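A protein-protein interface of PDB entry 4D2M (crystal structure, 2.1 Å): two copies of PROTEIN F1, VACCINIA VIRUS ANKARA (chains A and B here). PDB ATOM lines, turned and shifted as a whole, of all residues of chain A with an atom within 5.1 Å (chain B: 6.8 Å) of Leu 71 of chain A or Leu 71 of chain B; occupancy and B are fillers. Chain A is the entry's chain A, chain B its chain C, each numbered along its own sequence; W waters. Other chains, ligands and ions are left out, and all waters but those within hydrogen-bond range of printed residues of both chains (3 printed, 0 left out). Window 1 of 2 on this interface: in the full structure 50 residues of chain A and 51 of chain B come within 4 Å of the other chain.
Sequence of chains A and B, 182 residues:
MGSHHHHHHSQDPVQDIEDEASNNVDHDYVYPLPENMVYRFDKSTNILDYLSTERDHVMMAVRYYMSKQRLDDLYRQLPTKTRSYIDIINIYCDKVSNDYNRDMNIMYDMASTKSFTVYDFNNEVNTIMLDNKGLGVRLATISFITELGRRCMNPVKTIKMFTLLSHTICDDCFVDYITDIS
Water W3 lies within hydrogen-bond range of OH of Tyr 64 of chain A (2.5 Å) and OD1 of Asp 72 of chain B (2.7 Å). Water W1 lies within hydrogen-bond range of OD1 of Asp 72 of chain A (2.7 Å), OH of Tyr 64 of chain B (3.0 Å) and NZ of Lys 68 of chain B (3.1 Å). Water W2 bridges the backbone carbonyl oxygen of Gln 69 of chain A (2.7 Å) and the guanidinium group of Arg 150 of chain B (2.8 Å).
Tyr 64 of chain A touches Tyr 75 of chain B, and with the chains exchanged Tyr 75 of chain A touches Tyr 64 of chain B. Ser 67 of chain A touches Leu 71 of chain B, and with the chains exchanged Leu 71 of chain A touches Ser 67 of chain B. Lys 68 of chain B touches its own counterpart, Lys 68 of chain A. Lys 68 of chain A touches Leu 71 of chain B, and with the chains exchanged Leu 71 of chain A touches Lys 68 of chain B. 10 positions are printed for both chains. Of the 13 pairs that touch across the chains among the printed residues, 10 have their exchanged pair printed and touching as well.
Of the printed residues of chain B, Ser 67 of chain A touches Leu 71 (3.98 Å). Of chain B, only Tyr 64, Ser 67, Lys 68 and Leu 71 come within 4 Å of Leu 71 of chain A. Arg 63 of chain B touches none of the printed residues of chain A. Of the printed residues of chain A, Lys 68 of chain B touches Lys 68 (3.6 Å) and Leu 71 (3.6 Å). Printed residues of chain A within 4 Å of Leu 71 of chain B: Tyr 64 (3.5 Å), Ser 67 (3.98 Å), Lys 68 (3.8 Å) and Leu 71 (3.7 Å). Of the printed residues of chain A, Leu 74 of chain B touches Tyr 64. Of the printed residues of chain A, Tyr 75 of chain B touches Tyr 64. Arg 76 of chain B touches none of the printed residues of chain A. The nearest printed residue of chain A that does not touch Leu 71 of chain B is Gln 69 of chain A (6.1 Å). The nearest printed residue of chain A that does not touch Lys 68 of chain B is Asp 72 of chain A (4.6 Å).
OE1 of Gln 69 of chain A is in hydrogen-bond range of NH2 of Arg 150 of chain B (2.8 Å).
Leu 71 of chain B touches Tyr 64 of chain A. CD2 of Tyr 64 of chain A touches CD2 of Leu 74 of chain B, at 3.98 Å. Tyr 64 of chain A touches Tyr 75 of chain B (OH to CB, 3.5 Å). Lys 68 of chain A touches Lys 68 of chain B (CE to NZ, 3.6 Å). Leu 71 of chain B touches Lys 68 of chain A (CD2 to CA, 3.8 Å). Leu 71 of chain A touches Tyr 64 of chain B. CD2 of Leu 71 of chain A touches CA of Lys 68 of chain B, 3.6 Å away. Leu 71 of chain A touches Leu 71 of chain B. Asp 73 of chain A touches Arg 150 of chain B (OD2 to CB, 3.6 Å). OH of Tyr 64 of chain B touches CB of Tyr 75 of chain A, 3.4 Å away.
Of the 14 printed residues of chain B, 7 touch a printed residue of chain A. Hydrophobic or aromatic side chains of chain B that line the printed part of chain A: Tyr 64, Leu 71, Leu 74 and Tyr 75. Among the printed residues, 13 pairs touch across the chains. Among the printed residues, no Asp or Glu carboxylate lies within 4 Å of a Lys or Arg side-chain nitrogen of the other chain.
The backbone carbonyl oxygen of Arg 63 of chain B sits at hydrogen-bond distance from the side-chain hydroxyl of Ser 67 of chain B (3.1 Å). The side-chain amino group of Lys 68 of chain B is in salt-bridge range of the side-chain carboxylate of Asp 72 of chain B, at 3.8 Å. The side-chain amino group (NZ) of Lys 68 of chain A lies within salt-bridge range of the side-chain carboxylate (OD2) of Asp 72 of chain A, at 3.4 Å.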
ATOM      1  N   TYR A  64       6.429  -0.623  -8.524  1.00  0.00           N
ATOM      2  CA  TYR A  64       7.003   0.697  -8.293  1.00  0.00           C
ATOM      3  C   TYR A  64       8.007   0.643  -7.150  1.00  0.00           C
ATOM      4  O   TYR A  64       9.103   1.190  -7.250  1.00  0.00           O
ATOM      5  CB  TYR A  64       5.913   1.730  -7.985  1.00  0.00           C
ATOM      6  CG  TYR A  64       6.451   3.140  -7.862  1.00  0.00           C
ATOM      7  CD1 TYR A  64       6.950   3.613  -6.654  1.00  0.00           C
ATOM      8  CD2 TYR A  64       6.479   3.990  -8.957  1.00  0.00           C
ATOM      9  CE1 TYR A  64       7.453   4.898  -6.544  1.00  0.00           C
ATOM     10  CE2 TYR A  64       6.977   5.276  -8.855  1.00  0.00           C
ATOM     11  CZ  TYR A  64       7.463   5.723  -7.650  1.00  0.00           C
ATOM     12  OH  TYR A  64       7.957   7.002  -7.560  1.00  0.00           O
ATOM     13  N   SER A  67      11.295  -1.129  -8.192  1.00  0.00           N
ATOM     14  CA  SER A  67      12.096  -0.330  -9.112  1.00  0.00           C
ATOM     15  C   SER A  67      12.654   0.915  -8.427  1.00  0.00           C
ATOM     16  O   SER A  67      13.804   1.290  -8.644  1.00  0.00           O
ATOM     17  CB  SER A  67      11.265   0.072 -10.331  1.00  0.00           C
ATOM     18  OG  SER A  67      10.900  -1.061 -11.100  1.00  0.00           O
ATOM     19  N   LYS A  68      11.832   1.553  -7.601  1.00  0.00           N
ATOM     20  CA  LYS A  68      12.254   2.745  -6.879  1.00  0.00           C
ATOM     21  C   LYS A  68      13.385   2.401  -5.915  1.00  0.00           C
ATOM     22  O   LYS A  68      14.376   3.126  -5.824  1.00  0.00           O
ATOM     23  CB  LYS A  68      11.071   3.362  -6.130  1.00  0.00           C
ATOM     24  CG  LYS A  68      11.396   4.637  -5.355  1.00  0.00           C
ATOM     25  CD  LYS A  68      11.956   5.720  -6.261  1.00  0.00           C
ATOM     26  CE  LYS A  68      11.774   7.104  -5.655  1.00  0.00           C
ATOM     27  NZ  LYS A  68      12.280   7.189  -4.257  1.00  0.00           N
ATOM     28  N   GLN A  69      13.231   1.286  -5.207  1.00  0.00           N
ATOM     29  CA  GLN A  69      14.252   0.811  -4.282  1.00  0.00           C
ATOM     30  C   GLN A  69      15.563   0.533  -5.006  1.00  0.00           C
ATOM     31  O   GLN A  69      16.640   0.857  -4.503  1.00  0.00           O
ATOM     32  CB  GLN A  69      13.779  -0.456  -3.564  1.00  0.00           C
ATOM     33  CG  GLN A  69      12.810  -0.198  -2.430  1.00  0.00           C
ATOM     34  CD  GLN A  69      13.459   0.524  -1.267  1.00  0.00           C
ATOM     35  OE1 GLN A  69      14.519   0.125  -0.786  1.00  0.00           O
ATOM     36  NE2 GLN A  69      12.831   1.599  -0.816  1.00  0.00           N
ATOM     37  N   ARG A  70      15.467  -0.076  -6.183  1.00  0.00           N
ATOM     38  CA  ARG A  70      16.650  -0.361  -6.982  1.00  0.00           C
ATOM     39  C   ARG A  70      17.376   0.921  -7.367  1.00  0.00           C
ATOM     40  O   ARG A  70      18.599   1.013  -7.252  1.00  0.00           O
ATOM     41  CB  ARG A  70      16.277  -1.134  -8.242  1.00  0.00           C
ATOM     42  CG  ARG A  70      17.411  -1.221  -9.249  1.00  0.00           C
ATOM     43  CD  ARG A  70      16.957  -1.897 -10.512  1.00  0.00           C
ATOM     44  NE  ARG A  70      17.905  -1.690 -11.603  1.00  0.00           N
ATOM     45  CZ  ARG A  70      19.095  -2.276 -11.674  1.00  0.00           C
ATOM     46  NH1 ARG A  70      19.486  -3.101 -10.711  1.00  0.00           N
ATOM     47  NH2 ARG A  70      19.898  -2.035 -12.701  1.00  0.00           N
ATOM     48  N   LEU A  71      16.617   1.898  -7.853  1.00  0.00           N
ATOM     49  CA  LEU A  71      17.199   3.148  -8.321  1.00  0.00           C
ATOM     50  C   LEU A  71      17.836   3.907  -7.164  1.00  0.00           C
ATOM     51  O   LEU A  71      18.904   4.497  -7.316  1.00  0.00           O
ATOM     52  CB  LEU A  71      16.134   4.007  -9.008  1.00  0.00           C
ATOM     53  CG  LEU A  71      16.473   4.604 -10.379  1.00  0.00           C
ATOM     54  CD1 LEU A  71      17.005   3.568 -11.361  1.00  0.00           C
ATOM     55  CD2 LEU A  71      15.237   5.255 -10.965  1.00  0.00           C
ATOM     56  N   ASP A  72      17.179   3.882  -6.008  1.00  0.00           N
ATOM     57  CA  ASP A  72      17.719   4.502  -4.806  1.00  0.00           C
ATOM     58  C   ASP A  72      19.056   3.874  -4.424  1.00  0.00           C
ATOM     59  O   ASP A  72      20.024   4.579  -4.141  1.00  0.00           O
ATOM     60  CB  ASP A  72      16.732   4.374  -3.645  1.00  0.00           C
ATOM     61  CG  ASP A  72      15.550   5.318  -3.774  1.00  0.00           C
ATOM     62  OD1 ASP A  72      15.405   5.960  -4.834  1.00  0.00           O
ATOM     63  OD2 ASP A  72      14.759   5.411  -2.813  1.00  0.00           O
ATOM     64  N   ASP A  73      19.111   2.545  -4.428  1.00  0.00           N
ATOM     65  CA  ASP A  73      20.321   1.841  -4.022  1.00  0.00           C
ATOM     66  C   ASP A  73      21.428   2.004  -5.052  1.00  0.00           C
ATOM     67  O   ASP A  73      22.607   2.051  -4.701  1.00  0.00           O
ATOM     68  CB  ASP A  73      20.036   0.357  -3.801  1.00  0.00           C
ATOM     69  CG  ASP A  73      21.232  -0.383  -3.231  1.00  0.00           C
ATOM     70  OD1 ASP A  73      21.433  -0.331  -2.000  1.00  0.00           O
ATOM     71  OD2 ASP A  73      21.971  -1.014  -4.015  1.00  0.00           O
ATOM     72  N   LEU A  74      21.049   2.082  -6.322  1.00  0.00           N
ATOM     73  CA  LEU A  74      22.025   2.292  -7.382  1.00  0.00           C
ATOM     74  C   LEU A  74      22.710   3.643  -7.193  1.00  0.00           C
ATOM     75  O   LEU A  74      23.935   3.739  -7.253  1.00  0.00           O
ATOM     76  CB  LEU A  74      21.358   2.212  -8.757  1.00  0.00           C
ATOM     77  CG  LEU A  74      22.251   2.453  -9.977  1.00  0.00           C
ATOM     78  CD1 LEU A  74      23.472   1.543  -9.959  1.00  0.00           C
ATOM     79  CD2 LEU A  74      21.457   2.247 -11.265  1.00  0.00           C
ATOM     80  N   TYR A  75      21.916   4.680  -6.940  1.00  0.00           N
ATOM     81  CA  TYR A  75      22.456   6.022  -6.742  1.00  0.00           C
ATOM     82  C   TYR A  75      23.417   6.084  -5.553  1.00  0.00           C
ATOM     83  O   TYR A  75      24.455   6.740  -5.629  1.00  0.00           O
ATOM     84  CB  TYR A  75      21.325   7.033  -6.544  1.00  0.00           C
ATOM     85  CG  TYR A  75      21.787   8.473  -6.604  1.00  0.00           C
ATOM     86  CD1 TYR A  75      21.878   9.144  -7.819  1.00  0.00           C
ATOM     87  CD2 TYR A  75      22.138   9.161  -5.450  1.00  0.00           C
ATOM     88  CE1 TYR A  75      22.304  10.460  -7.879  1.00  0.00           C
ATOM     89  CE2 TYR A  75      22.563  10.474  -5.502  1.00  0.00           C
ATOM     90  CZ  TYR A  75      22.645  11.117  -6.719  1.00  0.00           C
ATOM     91  OH  TYR A  75      23.068  12.423  -6.774  1.00  0.00           O
ATOM     92  N   ARG B  63      21.208   6.561 -18.496  1.00  0.00           N
ATOM     93  CA  ARG B  63      20.239   5.526 -18.136  1.00  0.00           C
ATOM     94  C   ARG B  63      19.526   5.847 -16.825  1.00  0.00           C
ATOM     95  O   ARG B  63      18.317   5.645 -16.703  1.00  0.00           O
ATOM     96  CB  ARG B  63      20.920   4.162 -18.028  1.00  0.00           C
ATOM     97  CG  ARG B  63      21.421   3.613 -19.347  1.00  0.00           C
ATOM     98  CD  ARG B  63      21.948   2.191 -19.190  1.00  0.00           C
ATOM     99  NE  ARG B  63      23.109   1.942 -20.038  1.00  0.00           N
ATOM    100  CZ  ARG B  63      23.706   0.761 -20.172  1.00  0.00           C
ATOM    101  NH1 ARG B  63      23.252  -0.301 -19.519  1.00  0.00           N
ATOM    102  NH2 ARG B  63      24.759   0.641 -20.968  1.00  0.00           N
ATOM    103  N   TYR B  64      20.274   6.337 -15.840  1.00  0.00           N
ATOM    104  CA  TYR B  64      19.680   6.699 -14.558  1.00  0.00           C
ATOM    105  C   TYR B  64      18.633   7.787 -14.763  1.00  0.00           C
ATOM    106  O   TYR B  64      17.512   7.687 -14.263  1.00  0.00           O
ATOM    107  CB  TYR B  64      20.747   7.175 -13.566  1.00  0.00           C
ATOM    108  CG  TYR B  64      20.197   7.413 -12.175  1.00  0.00           C
ATOM    109  CD1 TYR B  64      19.658   8.643 -11.820  1.00  0.00           C
ATOM    110  CD2 TYR B  64      20.201   6.402 -11.226  1.00  0.00           C
ATOM    111  CE1 TYR B  64      19.147   8.859 -10.553  1.00  0.00           C
ATOM    112  CE2 TYR B  64      19.693   6.607  -9.962  1.00  0.00           C
ATOM    113  CZ  TYR B  64      19.166   7.836  -9.630  1.00  0.00           C
ATOM    114  OH  TYR B  64      18.660   8.036  -8.368  1.00  0.00           O
ATOM    115  N   MET B  66      16.972   8.709 -17.562  1.00  0.00           N
ATOM    116  CA  MET B  66      15.818   8.179 -18.280  1.00  0.00           C
ATOM    117  C   MET B  66      14.915   7.407 -17.326  1.00  0.00           C
ATOM    118  O   MET B  66      13.703   7.608 -17.295  1.00  0.00           O
ATOM    119  CB  MET B  66      16.262   7.272 -19.432  1.00  0.00           C
ATOM    120  CG  MET B  66      16.906   7.998 -20.600  1.00  0.00           C
ATOM    121  SD  MET B  66      17.543   6.849 -21.843  1.00  0.00           S
ATOM    122  CE  MET B  66      18.045   7.984 -23.135  1.00  0.00           C
ATOM    123  N   SER B  67      15.526   6.529 -16.541  1.00  0.00           N
ATOM    124  CA  SER B  67      14.792   5.677 -15.619  1.00  0.00           C
ATOM    125  C   SER B  67      14.128   6.474 -14.500  1.00  0.00           C
ATOM    126  O   SER B  67      12.970   6.233 -14.157  1.00  0.00           O
ATOM    127  CB  SER B  67      15.736   4.630 -15.031  1.00  0.00           C
ATOM    128  OG  SER B  67      16.031   3.631 -15.990  1.00  0.00           O
ATOM    129  N   LYS B  68      14.868   7.422 -13.933  1.00  0.00           N
ATOM    130  CA  LYS B  68      14.357   8.243 -12.842  1.00  0.00           C
ATOM    131  C   LYS B  68      13.170   9.084 -13.302  1.00  0.00           C
ATOM    132  O   LYS B  68      12.144   9.150 -12.622  1.00  0.00           O
ATOM    133  CB  LYS B  68      15.466   9.145 -12.295  1.00  0.00           C
ATOM    134  CG  LYS B  68      15.042  10.032 -11.130  1.00  0.00           C
ATOM    135  CD  LYS B  68      14.608   9.212  -9.926  1.00  0.00           C
ATOM    136  CE  LYS B  68      14.283  10.101  -8.736  1.00  0.00           C
ATOM    137  NZ  LYS B  68      13.840   9.310  -7.557  1.00  0.00           N
ATOM    138  N   GLN B  69      13.324   9.724 -14.458  1.00  0.00           N
ATOM    139  CA  GLN B  69      12.263  10.531 -15.054  1.00  0.00           C
ATOM    140  C   GLN B  69      10.991   9.720 -15.268  1.00  0.00           C
ATOM    141  O   GLN B  69       9.886  10.206 -15.018  1.00  0.00           O
ATOM    142  CB  GLN B  69      12.728  11.115 -16.391  1.00  0.00           C
ATOM    143  CG  GLN B  69      13.649  12.313 -16.265  1.00  0.00           C
ATOM    144  CD  GLN B  69      12.958  13.515 -15.647  1.00  0.00           C
ATOM    145  OE1 GLN B  69      11.864  13.897 -16.059  1.00  0.00           O
ATOM    146  NE2 GLN B  69      13.594  14.111 -14.647  1.00  0.00           N
ATOM    147  N   ARG B  70      11.150   8.487 -15.738  1.00  0.00           N
ATOM    148  CA  ARG B  70      10.007   7.617 -15.982  1.00  0.00           C
ATOM    149  C   ARG B  70       9.260   7.328 -14.688  1.00  0.00           C
ATOM    150  O   ARG B  70       8.035   7.395 -14.638  1.00  0.00           O
ATOM    151  CB  ARG B  70      10.451   6.306 -16.626  1.00  0.00           C
ATOM    152  CG  ARG B  70       9.368   5.243 -16.647  1.00  0.00           C
ATOM    153  CD  ARG B  70       9.888   3.968 -17.254  1.00  0.00           C
ATOM    154  NE  ARG B  70       8.974   2.848 -17.048  1.00  0.00           N
ATOM    155  CZ  ARG B  70       7.811   2.707 -17.678  1.00  0.00           C
ATOM    156  NH1 ARG B  70       7.413   3.623 -18.550  1.00  0.00           N
ATOM    157  NH2 ARG B  70       7.044   1.653 -17.430  1.00  0.00           N
ATOM    158  N   LEU B  71      10.012   6.982 -13.649  1.00  0.00           N
ATOM    159  CA  LEU B  71       9.426   6.654 -12.357  1.00  0.00           C
ATOM    160  C   LEU B  71       8.709   7.859 -11.752  1.00  0.00           C
ATOM    161  O   LEU B  71       7.608   7.725 -11.220  1.00  0.00           O
ATOM    162  CB  LEU B  71      10.509   6.149 -11.401  1.00  0.00           C
ATOM    163  CG  LEU B  71      10.399   4.720 -10.860  1.00  0.00           C
ATOM    164  CD1 LEU B  71       9.957   3.704 -11.907  1.00  0.00           C
ATOM    165  CD2 LEU B  71      11.746   4.311 -10.303  1.00  0.00           C
ATOM    166  N   ASP B  72       9.334   9.031 -11.840  1.00  0.00           N
ATOM    167  CA  ASP B  72       8.735  10.260 -11.326  1.00  0.00           C
ATOM    168  C   ASP B  72       7.417  10.573 -12.027  1.00  0.00           C
ATOM    169  O   ASP B  72       6.436  10.945 -11.383  1.00  0.00           O
ATOM    170  CB  ASP B  72       9.695  11.441 -11.490  1.00  0.00           C
ATOM    171  CG  ASP B  72      10.857  11.393 -10.516  1.00  0.00           C
ATOM    172  OD1 ASP B  72      10.845  10.543  -9.601  1.00  0.00           O
ATOM    173  OD2 ASP B  72      11.782  12.220 -10.660  1.00  0.00           O
ATOM    174  N   ASP B  73       7.397  10.417 -13.347  1.00  0.00           N
ATOM    175  CA  ASP B  73       6.210  10.742 -14.125  1.00  0.00           C
ATOM    176  C   ASP B  73       5.120   9.690 -13.940  1.00  0.00           C
ATOM    177  O   ASP B  73       3.932  10.004 -14.001  1.00  0.00           O
ATOM    178  CB  ASP B  73       6.556  10.881 -15.606  1.00  0.00           C
ATOM    179  CG  ASP B  73       5.435  11.514 -16.402  1.00  0.00           C
ATOM    180  OD1 ASP B  73       5.330  12.758 -16.393  1.00  0.00           O
ATOM    181  OD2 ASP B  73       4.656  10.768 -17.030  1.00  0.00           O
ATOM    182  N   LEU B  74       5.525   8.443 -13.723  1.00  0.00           N
ATOM    183  CA  LEU B  74       4.571   7.382 -13.422  1.00  0.00           C
ATOM    184  C   LEU B  74       3.833   7.697 -12.124  1.00  0.00           C
ATOM    185  O   LEU B  74       2.604   7.667 -12.075  1.00  0.00           O
ATOM    186  CB  LEU B  74       5.276   6.028 -13.314  1.00  0.00           C
ATOM    187  CG  LEU B  74       4.414   4.861 -12.819  1.00  0.00           C
ATOM    188  CD1 LEU B  74       3.209   4.644 -13.727  1.00  0.00           C
ATOM    189  CD2 LEU B  74       5.242   3.590 -12.717  1.00  0.00           C
ATOM    190  N   TYR B  75       4.593   7.997 -11.076  1.00  0.00           N
ATOM    191  CA  TYR B  75       4.015   8.326  -9.779  1.00  0.00           C
ATOM    192  C   TYR B  75       3.104   9.542  -9.891  1.00  0.00           C
ATOM    193  O   TYR B  75       2.053   9.606  -9.256  1.00  0.00           O
ATOM    194  CB  TYR B  75       5.114   8.591  -8.752  1.00  0.00           C
ATOM    195  CG  TYR B  75       4.594   8.713  -7.343  1.00  0.00           C
ATOM    196  CD1 TYR B  75       4.431   7.590  -6.547  1.00  0.00           C
ATOM    197  CD2 TYR B  75       4.258   9.950  -6.810  1.00  0.00           C
ATOM    198  CE1 TYR B  75       3.953   7.691  -5.258  1.00  0.00           C
ATOM    199  CE2 TYR B  75       3.777  10.061  -5.519  1.00  0.00           C
ATOM    200  CZ  TYR B  75       3.627   8.926  -4.749  1.00  0.00           C
ATOM    201  OH  TYR B  75       3.149   9.020  -3.462  1.00  0.00           O
ATOM    202  N   ARG B  76       3.525  10.501 -10.706  1.00  0.00           N
ATOM    203  CA  ARG B  76       2.749  11.708 -10.955  1.00  0.00           C
ATOM    204  C   ARG B  76       1.352  11.367 -11.469  1.00  0.00           C
ATOM    205  O   ARG B  76       0.385  12.075 -11.184  1.00  0.00           O
ATOM    206  CB  ARG B  76       3.480  12.596 -11.962  1.00  0.00           C
ATOM    207  CG  ARG B  76       3.117  14.069 -11.888  1.00  0.00           C
ATOM    208  CD  ARG B  76       3.730  14.845 -13.044  1.00  0.00           C
ATOM    209  NE  ARG B  76       3.355  14.278 -14.337  1.00  0.00           N
ATOM    210  CZ  ARG B  76       2.178  14.463 -14.926  1.00  0.00           C
ATOM    211  NH1 ARG B  76       1.246  15.206 -14.343  1.00  0.00           N
ATOM    212  NH2 ARG B  76       1.929  13.902 -16.101  1.00  0.00           N
ATOM    213  N   ARG B 150      18.684  -4.941  -6.145  1.00  0.00           N
ATOM    214  CA  ARG B 150      19.739  -4.004  -5.768  1.00  0.00           C
ATOM    215  C   ARG B 150      21.122  -4.472  -6.214  1.00  0.00           C
ATOM    216  O   ARG B 150      22.025  -3.656  -6.405  1.00  0.00           O
ATOM    217  CB  ARG B 150      19.754  -3.787  -4.250  1.00  0.00           C
ATOM    218  CG  ARG B 150      18.532  -3.082  -3.680  1.00  0.00           C
ATOM    219  CD  ARG B 150      18.742  -2.750  -2.203  1.00  0.00           C
ATOM    220  NE  ARG B 150      17.531  -2.234  -1.564  1.00  0.00           N
ATOM    221  CZ  ARG B 150      16.664  -2.969  -0.871  1.00  0.00           C
ATOM    222  NH1 ARG B 150      16.854  -4.273  -0.709  1.00  0.00           N
ATOM    223  NH2 ARG B 150      15.596  -2.394  -0.334  1.00  0.00           N
HETATM  224  O   HOH W   1      16.044   7.096  -7.172  1.00  0.00           O
HETATM  225  O   HOH W   2      17.159   0.505  -1.842  1.00  0.00           O
HETATM  226  O   HOH W   3       9.772   8.454  -8.348  1.00  0.00           O
